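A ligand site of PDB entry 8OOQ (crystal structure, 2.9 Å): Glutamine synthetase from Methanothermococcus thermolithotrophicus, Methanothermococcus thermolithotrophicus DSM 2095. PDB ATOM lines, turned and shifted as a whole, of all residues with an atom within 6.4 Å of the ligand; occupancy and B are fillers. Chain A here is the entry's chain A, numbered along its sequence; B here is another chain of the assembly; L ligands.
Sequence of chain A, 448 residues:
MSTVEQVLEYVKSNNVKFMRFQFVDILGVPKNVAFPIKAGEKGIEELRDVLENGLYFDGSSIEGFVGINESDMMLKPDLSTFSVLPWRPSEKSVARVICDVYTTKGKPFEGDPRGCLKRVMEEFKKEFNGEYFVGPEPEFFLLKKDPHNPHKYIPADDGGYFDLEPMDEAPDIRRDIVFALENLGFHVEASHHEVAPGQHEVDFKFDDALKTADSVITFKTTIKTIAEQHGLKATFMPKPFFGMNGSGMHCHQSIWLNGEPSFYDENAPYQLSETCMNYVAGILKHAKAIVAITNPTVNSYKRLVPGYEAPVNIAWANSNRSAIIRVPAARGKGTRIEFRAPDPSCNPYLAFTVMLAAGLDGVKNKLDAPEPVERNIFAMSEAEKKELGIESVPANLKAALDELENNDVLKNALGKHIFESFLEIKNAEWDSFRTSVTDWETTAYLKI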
ATOM      1  N   GLU A 165      11.177 -21.708   2.668  1.00  0.00           N
ATOM      2  CA  GLU A 165      12.467 -21.277   3.221  1.00  0.00           C
ATOM      3  C   GLU A 165      13.286 -22.513   3.687  1.00  0.00           C
ATOM      4  O   GLU A 165      12.688 -23.515   4.085  1.00  0.00           O
ATOM      5  CB  GLU A 165      12.269 -20.291   4.384  1.00  0.00           C
ATOM      6  CG  GLU A 165      11.342 -20.747   5.520  1.00  0.00           C
ATOM      7  CD  GLU A 165       9.855 -20.514   5.344  1.00  0.00           C
ATOM      8  OE1 GLU A 165       9.441 -20.085   4.243  1.00  0.00           O
ATOM      9  OE2 GLU A 165       9.096 -20.787   6.300  1.00  0.00           O
ATOM     10  N   ASP A 168      13.511 -20.310  -0.433  1.00  0.00           N
ATOM     11  CA  ASP A 168      12.853 -19.023  -0.610  1.00  0.00           C
ATOM     12  C   ASP A 168      13.387 -18.131   0.516  1.00  0.00           C
ATOM     13  O   ASP A 168      13.088 -18.394   1.677  1.00  0.00           O
ATOM     14  CB  ASP A 168      11.314 -19.185  -0.499  1.00  0.00           C
ATOM     15  CG  ASP A 168      10.534 -17.899  -0.265  1.00  0.00           C
ATOM     16  OD1 ASP A 168      10.904 -16.867  -0.872  1.00  0.00           O
ATOM     17  OD2 ASP A 168       9.562 -17.930   0.517  1.00  0.00           O
ATOM     18  N   ALA A 170      12.677 -14.888   0.923  1.00  0.00           N
ATOM     19  CA  ALA A 170      11.853 -13.688   1.070  1.00  0.00           C
ATOM     20  C   ALA A 170      10.597 -13.849   1.953  1.00  0.00           C
ATOM     21  O   ALA A 170       9.671 -13.056   1.755  1.00  0.00           O
ATOM     22  CB  ALA A 170      11.476 -13.173  -0.311  1.00  0.00           C
ATOM     23  N   PRO A 171      10.510 -14.788   2.934  1.00  0.00           N
ATOM     24  CA  PRO A 171       9.316 -14.814   3.792  1.00  0.00           C
ATOM     25  C   PRO A 171       9.279 -13.628   4.768  1.00  0.00           C
ATOM     26  O   PRO A 171       8.203 -13.178   5.131  1.00  0.00           O
ATOM     27  CB  PRO A 171       9.431 -16.150   4.538  1.00  0.00           C
ATOM     28  CG  PRO A 171      10.631 -16.842   3.987  1.00  0.00           C
ATOM     29  CD  PRO A 171      11.489 -15.789   3.374  1.00  0.00           C
ATOM     30  N   ASP A 172      10.458 -13.097   5.162  1.00  0.00           N
ATOM     31  CA  ASP A 172      10.537 -11.936   6.043  1.00  0.00           C
ATOM     32  C   ASP A 172      10.119 -10.673   5.306  1.00  0.00           C
ATOM     33  O   ASP A 172       9.450  -9.837   5.893  1.00  0.00           O
ATOM     34  CB  ASP A 172      11.979 -11.765   6.563  1.00  0.00           C
ATOM     35  CG  ASP A 172      12.450 -12.875   7.459  1.00  0.00           C
ATOM     36  OD1 ASP A 172      11.765 -13.156   8.473  1.00  0.00           O
ATOM     37  OD2 ASP A 172      13.515 -13.467   7.170  1.00  0.00           O
ATOM     38  N   ARG A 174       8.172 -10.465   2.463  1.00  0.00           N
ATOM     39  CA  ARG A 174       6.743 -10.542   2.126  1.00  0.00           C
ATOM     40  C   ARG A 174       5.873 -10.349   3.383  1.00  0.00           C
ATOM     41  O   ARG A 174       4.761  -9.835   3.259  1.00  0.00           O
ATOM     42  CB  ARG A 174       6.390 -11.851   1.401  1.00  0.00           C
ATOM     43  CG  ARG A 174       6.953 -11.932  -0.024  1.00  0.00           C
ATOM     44  CD  ARG A 174       6.235 -12.984  -0.850  1.00  0.00           C
ATOM     45  NE  ARG A 174       6.262 -14.313  -0.233  1.00  0.00           N
ATOM     46  CZ  ARG A 174       7.310 -15.139  -0.232  1.00  0.00           C
ATOM     47  NH1 ARG A 174       8.453 -14.785  -0.815  1.00  0.00           N
ATOM     48  NH2 ARG A 174       7.219 -16.321   0.367  1.00  0.00           N
ATOM     49  N   ARG A 175       6.370 -10.698   4.583  1.00  0.00           N
ATOM     50  CA  ARG A 175       5.650 -10.488   5.843  1.00  0.00           C
ATOM     51  C   ARG A 175       5.376  -8.996   6.041  1.00  0.00           C
ATOM     52  O   ARG A 175       4.244  -8.613   6.317  1.00  0.00           O
ATOM     53  CB  ARG A 175       6.481 -11.025   7.037  1.00  0.00           C
ATOM     54  CG  ARG A 175       5.827 -10.904   8.413  1.00  0.00           C
ATOM     55  CD  ARG A 175       6.829 -11.243   9.512  1.00  0.00           C
ATOM     56  NE  ARG A 175       6.295 -11.061  10.858  1.00  0.00           N
ATOM     57  CZ  ARG A 175       5.493 -11.912  11.502  1.00  0.00           C
ATOM     58  NH1 ARG A 175       5.091 -13.030  10.918  1.00  0.00           N
ATOM     59  NH2 ARG A 175       5.083 -11.636  12.734  1.00  0.00           N
ATOM     60  N   ASP A 176       6.394  -8.156   5.843  1.00  0.00           N
ATOM     61  CA  ASP A 176       6.270  -6.708   6.009  1.00  0.00           C
ATOM     62  C   ASP A 176       5.491  -6.052   4.867  1.00  0.00           C
ATOM     63  O   ASP A 176       4.789  -5.087   5.115  1.00  0.00           O
ATOM     64  CB  ASP A 176       7.652  -6.063   6.169  1.00  0.00           C
ATOM     65  CG  ASP A 176       8.430  -6.599   7.353  1.00  0.00           C
ATOM     66  OD1 ASP A 176       7.796  -7.101   8.315  1.00  0.00           O
ATOM     67  OD2 ASP A 176       9.678  -6.527   7.335  1.00  0.00           O
ATOM     68  N   VAL A 178       2.951  -7.432   3.257  1.00  0.00           N
ATOM     69  CA  VAL A 178       1.548  -7.725   3.540  1.00  0.00           C
ATOM     70  C   VAL A 178       1.034  -6.833   4.674  1.00  0.00           C
ATOM     71  O   VAL A 178      -0.078  -6.313   4.562  1.00  0.00           O
ATOM     72  CB  VAL A 178       1.334  -9.226   3.833  1.00  0.00           C
ATOM     73  CG1 VAL A 178      -0.091  -9.482   4.300  1.00  0.00           C
ATOM     74  CG2 VAL A 178       1.652 -10.086   2.605  1.00  0.00           C
ATOM     75  N   ALA A 190      -3.287 -13.532  -1.030  1.00  0.00           N
ATOM     76  CA  ALA A 190      -2.211 -14.529  -1.027  1.00  0.00           C
ATOM     77  C   ALA A 190      -0.853 -13.864  -1.282  1.00  0.00           C
ATOM     78  O   ALA A 190      -0.776 -12.778  -1.857  1.00  0.00           O
ATOM     79  CB  ALA A 190      -2.467 -15.598  -2.088  1.00  0.00           C
ATOM     80  N   SER A 191       0.219 -14.514  -0.834  1.00  0.00           N
ATOM     81  CA  SER A 191       1.576 -14.012  -1.044  1.00  0.00           C
ATOM     82  C   SER A 191       2.502 -15.223  -1.162  1.00  0.00           C
ATOM     83  O   SER A 191       2.429 -16.134  -0.338  1.00  0.00           O
ATOM     84  CB  SER A 191       1.991 -13.083   0.102  1.00  0.00           C
ATOM     85  OG  SER A 191       1.819 -13.701   1.368  1.00  0.00           O
ATOM     86  N   HIS A 192       3.327 -15.265  -2.215  1.00  0.00           N
ATOM     87  CA  HIS A 192       4.173 -16.424  -2.470  1.00  0.00           C
ATOM     88  C   HIS A 192       5.309 -16.110  -3.458  1.00  0.00           C
ATOM     89  O   HIS A 192       5.343 -15.038  -4.059  1.00  0.00           O
ATOM     90  CB  HIS A 192       3.300 -17.546  -3.048  1.00  0.00           C
ATOM     91  CG  HIS A 192       2.565 -17.160  -4.298  1.00  0.00           C
ATOM     92  ND1 HIS A 192       3.130 -17.314  -5.548  1.00  0.00           N
ATOM     93  CD2 HIS A 192       1.311 -16.647  -4.448  1.00  0.00           C
ATOM     94  CE1 HIS A 192       2.223 -16.889  -6.412  1.00  0.00           C
ATOM     95  NE2 HIS A 192       1.117 -16.478  -5.796  1.00  0.00           N
ATOM     96  N   HIS A 193       6.242 -17.055  -3.625  1.00  0.00           N
ATOM     97  CA  HIS A 193       7.343 -16.944  -4.583  1.00  0.00           C
ATOM     98  C   HIS A 193       6.815 -17.374  -5.963  1.00  0.00           C
ATOM     99  O   HIS A 193       5.907 -18.207  -6.048  1.00  0.00           O
ATOM    100  CB  HIS A 193       8.513 -17.863  -4.149  1.00  0.00           C
ATOM    101  CG  HIS A 193       9.842 -17.490  -4.721  1.00  0.00           C
ATOM    102  ND1 HIS A 193      10.132 -17.671  -6.064  1.00  0.00           N
ATOM    103  CD2 HIS A 193      10.945 -17.002  -4.103  1.00  0.00           C
ATOM    104  CE1 HIS A 193      11.387 -17.282  -6.222  1.00  0.00           C
ATOM    105  NE2 HIS A 193      11.914 -16.873  -5.078  1.00  0.00           N
ATOM    106  N   GLU A 201       5.122 -12.699  -5.754  1.00  0.00           N
ATOM    107  CA  GLU A 201       3.764 -12.298  -6.090  1.00  0.00           C
ATOM    108  C   GLU A 201       2.961 -12.048  -4.802  1.00  0.00           C
ATOM    109  O   GLU A 201       3.061 -12.826  -3.853  1.00  0.00           O
ATOM    110  CB  GLU A 201       3.098 -13.407  -6.929  1.00  0.00           C
ATOM    111  CG  GLU A 201       1.788 -13.005  -7.593  1.00  0.00           C
ATOM    112  CD  GLU A 201       1.143 -14.088  -8.442  1.00  0.00           C
ATOM    113  OE1 GLU A 201       1.870 -14.918  -9.030  1.00  0.00           O
ATOM    114  OE2 GLU A 201      -0.112 -14.091  -8.523  1.00  0.00           O
ATOM    115  N   PHE B  18      -0.660 -15.466   9.801  1.00  0.00           N
ATOM    116  CA  PHE B  18      -0.516 -16.084   8.476  1.00  0.00           C
ATOM    117  C   PHE B  18      -0.827 -17.569   8.507  1.00  0.00           C
ATOM    118  O   PHE B  18      -0.497 -18.237   9.484  1.00  0.00           O
ATOM    119  CB  PHE B  18       0.900 -15.868   7.949  1.00  0.00           C
ATOM    120  CG  PHE B  18       1.235 -14.420   7.681  1.00  0.00           C
ATOM    121  CD1 PHE B  18       0.874 -13.814   6.500  1.00  0.00           C
ATOM    122  CD2 PHE B  18       1.935 -13.678   8.620  1.00  0.00           C
ATOM    123  CE1 PHE B  18       1.184 -12.475   6.261  1.00  0.00           C
ATOM    124  CE2 PHE B  18       2.255 -12.354   8.365  1.00  0.00           C
ATOM    125  CZ  PHE B  18       1.876 -11.760   7.197  1.00  0.00           C
ATOM    126  N   MET B  19      -1.443 -18.082   7.428  1.00  0.00           N
ATOM    127  CA  MET B  19      -1.789 -19.501   7.293  1.00  0.00           C
ATOM    128  C   MET B  19      -1.143 -20.028   6.010  1.00  0.00           C
ATOM    129  O   MET B  19      -1.526 -19.631   4.916  1.00  0.00           O
ATOM    130  CB  MET B  19      -3.319 -19.670   7.246  1.00  0.00           C
ATOM    131  CG  MET B  19      -3.792 -21.114   7.256  1.00  0.00           C
ATOM    132  SD  MET B  19      -3.456 -21.997   8.790  1.00  0.00           S
ATOM    133  CE  MET B  19      -4.766 -21.356   9.812  1.00  0.00           C
ATOM    134  N   ARG B  20      -0.145 -20.913   6.149  1.00  0.00           N
ATOM    135  CA  ARG B  20       0.579 -21.503   5.032  1.00  0.00           C
ATOM    136  C   ARG B  20      -0.163 -22.755   4.580  1.00  0.00           C
ATOM    137  O   ARG B  20      -0.346 -23.677   5.383  1.00  0.00           O
ATOM    138  CB  ARG B  20       2.000 -21.907   5.470  1.00  0.00           C
ATOM    139  CG  ARG B  20       2.851 -20.817   6.098  1.00  0.00           C
ATOM    140  CD  ARG B  20       3.355 -19.792   5.106  1.00  0.00           C
ATOM    141  NE  ARG B  20       4.531 -19.066   5.587  1.00  0.00           N
ATOM    142  CZ  ARG B  20       5.785 -19.549   5.594  1.00  0.00           C
ATOM    143  NH1 ARG B  20       6.034 -20.775   5.162  1.00  0.00           N
ATOM    144  NH2 ARG B  20       6.779 -18.808   6.065  1.00  0.00           N
ATOM    145  N   VAL B  33       1.602 -21.519   0.017  1.00  0.00           N
ATOM    146  CA  VAL B  33       1.129 -20.160  -0.240  1.00  0.00           C
ATOM    147  C   VAL B  33       0.617 -19.595   1.084  1.00  0.00           C
ATOM    148  O   VAL B  33      -0.115 -20.277   1.805  1.00  0.00           O
ATOM    149  CB  VAL B  33       0.058 -20.097  -1.348  1.00  0.00           C
ATOM    150  CG1 VAL B  33      -1.085 -21.080  -1.100  1.00  0.00           C
ATOM    151  CG2 VAL B  33      -0.490 -18.673  -1.502  1.00  0.00           C
ATOM    152  N   ALA B  34       1.005 -18.355   1.433  1.00  0.00           N
ATOM    153  CA  ALA B  34       0.597 -17.740   2.685  1.00  0.00           C
ATOM    154  C   ALA B  34      -0.692 -16.932   2.510  1.00  0.00           C
ATOM    155  O   ALA B  34      -0.841 -16.203   1.535  1.00  0.00           O
ATOM    156  CB  ALA B  34       1.702 -16.830   3.202  1.00  0.00           C
ATOM    157  N   PHE B  35      -1.610 -17.064   3.465  1.00  0.00           N
ATOM    158  CA  PHE B  35      -2.883 -16.360   3.457  1.00  0.00           C
ATOM    159  C   PHE B  35      -2.904 -15.474   4.704  1.00  0.00           C
ATOM    160  O   PHE B  35      -2.798 -16.012   5.812  1.00  0.00           O
ATOM    161  CB  PHE B  35      -4.049 -17.363   3.490  1.00  0.00           C
ATOM    162  CG  PHE B  35      -5.391 -16.730   3.771  1.00  0.00           C
ATOM    163  CD1 PHE B  35      -6.040 -15.976   2.813  1.00  0.00           C
ATOM    164  CD2 PHE B  35      -5.986 -16.863   5.009  1.00  0.00           C
ATOM    165  CE1 PHE B  35      -7.264 -15.375   3.087  1.00  0.00           C
ATOM    166  CE2 PHE B  35      -7.210 -16.262   5.283  1.00  0.00           C
ATOM    167  CZ  PHE B  35      -7.839 -15.528   4.318  1.00  0.00           C
ATOM    168  N   LEU B  85       4.832 -22.575  13.170  1.00  0.00           N
ATOM    169  CA  LEU B  85       6.230 -22.640  12.768  1.00  0.00           C
ATOM    170  C   LEU B  85       7.066 -21.943  13.844  1.00  0.00           C
ATOM    171  O   LEU B  85       6.865 -20.763  14.105  1.00  0.00           O
ATOM    172  CB  LEU B  85       6.442 -21.958  11.407  1.00  0.00           C
ATOM    173  CG  LEU B  85       5.536 -22.438  10.254  1.00  0.00           C
ATOM    174  CD1 LEU B  85       5.905 -21.739   8.973  1.00  0.00           C
ATOM    175  CD2 LEU B  85       5.609 -23.950  10.059  1.00  0.00           C
ATOM    176  N   ARG B  88       9.572 -18.974  12.866  1.00  0.00           N
ATOM    177  CA  ARG B  88       8.918 -17.697  12.555  1.00  0.00           C
ATOM    178  C   ARG B  88       8.614 -16.907  13.874  1.00  0.00           C
ATOM    179  O   ARG B  88       8.730 -17.482  14.968  1.00  0.00           O
ATOM    180  CB  ARG B  88       7.634 -17.955  11.737  1.00  0.00           C
ATOM    181  CG  ARG B  88       7.851 -18.680  10.397  1.00  0.00           C
ATOM    182  CD  ARG B  88       8.835 -17.997   9.459  1.00  0.00           C
ATOM    183  NE  ARG B  88       8.473 -16.600   9.235  1.00  0.00           N
ATOM    184  CZ  ARG B  88       9.312 -15.586   8.998  1.00  0.00           C
ATOM    185  NH1 ARG B  88      10.631 -15.791   8.967  1.00  0.00           N
ATOM    186  NH2 ARG B  88       8.853 -14.358   8.797  1.00  0.00           N
ATOM    187  N   PRO B  89       8.239 -15.614  13.815  1.00  0.00           N
ATOM    188  CA  PRO B  89       7.989 -14.857  15.065  1.00  0.00           C
ATOM    189  C   PRO B  89       6.847 -15.379  15.917  1.00  0.00           C
ATOM    190  O   PRO B  89       5.925 -16.017  15.420  1.00  0.00           O
ATOM    191  CB  PRO B  89       7.718 -13.429  14.577  1.00  0.00           C
ATOM    192  CG  PRO B  89       8.278 -13.376  13.203  1.00  0.00           C
ATOM    193  CD  PRO B  89       8.073 -14.737  12.641  1.00  0.00           C
ATOM    194  N   LYS B  92       2.201 -12.304  16.369  1.00  0.00           N
ATOM    195  CA  LYS B  92       1.663 -12.334  15.005  1.00  0.00           C
ATOM    196  C   LYS B  92       2.245 -13.574  14.310  1.00  0.00           C
ATOM    197  O   LYS B  92       2.809 -13.486  13.228  1.00  0.00           O
ATOM    198  CB  LYS B  92       1.942 -11.042  14.226  1.00  0.00           C
ATOM    199  CG  LYS B  92       1.399  -9.807  14.932  1.00  0.00           C
ATOM    200  CD  LYS B  92       1.337  -8.617  13.989  1.00  0.00           C
ATOM    201  CE  LYS B  92       0.985  -7.343  14.721  1.00  0.00           C
ATOM    202  NZ  LYS B  92       0.733  -6.213  13.783  1.00  0.00           N
ATOM    203  N   VAL B  94       2.974 -17.418  12.637  1.00  0.00           N
ATOM    204  CA  VAL B  94       2.672 -18.038  11.356  1.00  0.00           C
ATOM    205  C   VAL B  94       2.296 -19.498  11.629  1.00  0.00           C
ATOM    206  O   VAL B  94       3.019 -20.183  12.345  1.00  0.00           O
ATOM    207  CB  VAL B  94       3.901 -17.952  10.427  1.00  0.00           C
ATOM    208  CG1 VAL B  94       3.621 -18.596   9.073  1.00  0.00           C
ATOM    209  CG2 VAL B  94       4.350 -16.500  10.267  1.00  0.00           C
HETATM  210  C1  LIG L   1       5.827 -15.317   7.214  1.00  0.00           C
HETATM  211  O1  LIG L   1       6.061 -14.334   7.958  1.00  0.00           O
HETATM  212  O2  LIG L   1       6.399 -16.408   7.384  1.00  0.00           O
HETATM  213  C2  LIG L   1       4.843 -15.187   6.142  1.00  0.00           C
HETATM  214  O3  LIG L   1       4.159 -16.152   5.840  1.00  0.00           O
HETATM  215  C3  LIG L   1       4.703 -13.856   5.429  1.00  0.00           C
HETATM  216  C4  LIG L   1       3.961 -13.961   4.100  1.00  0.00           C
HETATM  217  C5  LIG L   1       4.714 -14.731   3.043  1.00  0.00           C
HETATM  218  O4  LIG L   1       4.190 -14.856   1.926  1.00  0.00           O
HETATM  219  O5  LIG L   1       5.838 -15.223   3.289  1.00  0.00           O
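An oxygen (O2) of the ligand lies within salt-bridge range of the guanidinium group (NE) of Arg 88 of chain B. An oxygen (O2) of the ligand is in salt-bridge range of the guanidinium group (NH2) of Arg 20 of chain B, at 2.8 Å. An oxygen (O1) of the ligand is in salt-bridge range of the guanidinium group of Arg 175 (3.4 Å). NE of Arg 174 lies within salt-bridge range of O4 of the ligand, 3.0 Å away. The side-chain hydroxyl (OG) of Ser 191 sits at hydrogen-bond distance from an oxygen (O4) of the ligand (2.7 Å).
O of Val 94 of chain B is in hydrogen-bond range of N of Leu 85 of chain B (3.1 Å). NH1 of Arg 174 is in hydrogen-bond range of O of Ala 170, at 3.3 Å. The guanidinium group (NH1) of Arg 88 of chain B lies within salt-bridge range of the side-chain carboxylate (OD1) of Asp 172 (2.9 Å). NH2 of Arg 20 of chain B lies within salt-bridge range of OE2 of Glu 165 (3.1 Å). The backbone carbonyl oxygen of Lys 92 of chain B lies within hydrogen-bond range of the guanidinium group of Arg 175 (3.0 Å). N of Ser 191 is in hydrogen-bond range of O of Ala 34 of chain B, at 3.1 Å. The guanidinium group (NH2) of Arg 174 lies within salt-bridge range of the side-chain carboxylate (OD2) of Asp 168 (2.8 Å).
Pro 171 touches the ligand. Phe 18 of chain B touches the ligand. Ala 34 of chain B touches the ligand. Val 94 of chain B touches the ligand. Hydrophobic or aromatic side chains within 4 Å of the ligand: Pro 171, Phe 18 of chain B, Ala 34 of chain B and Val 94 of chain B.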
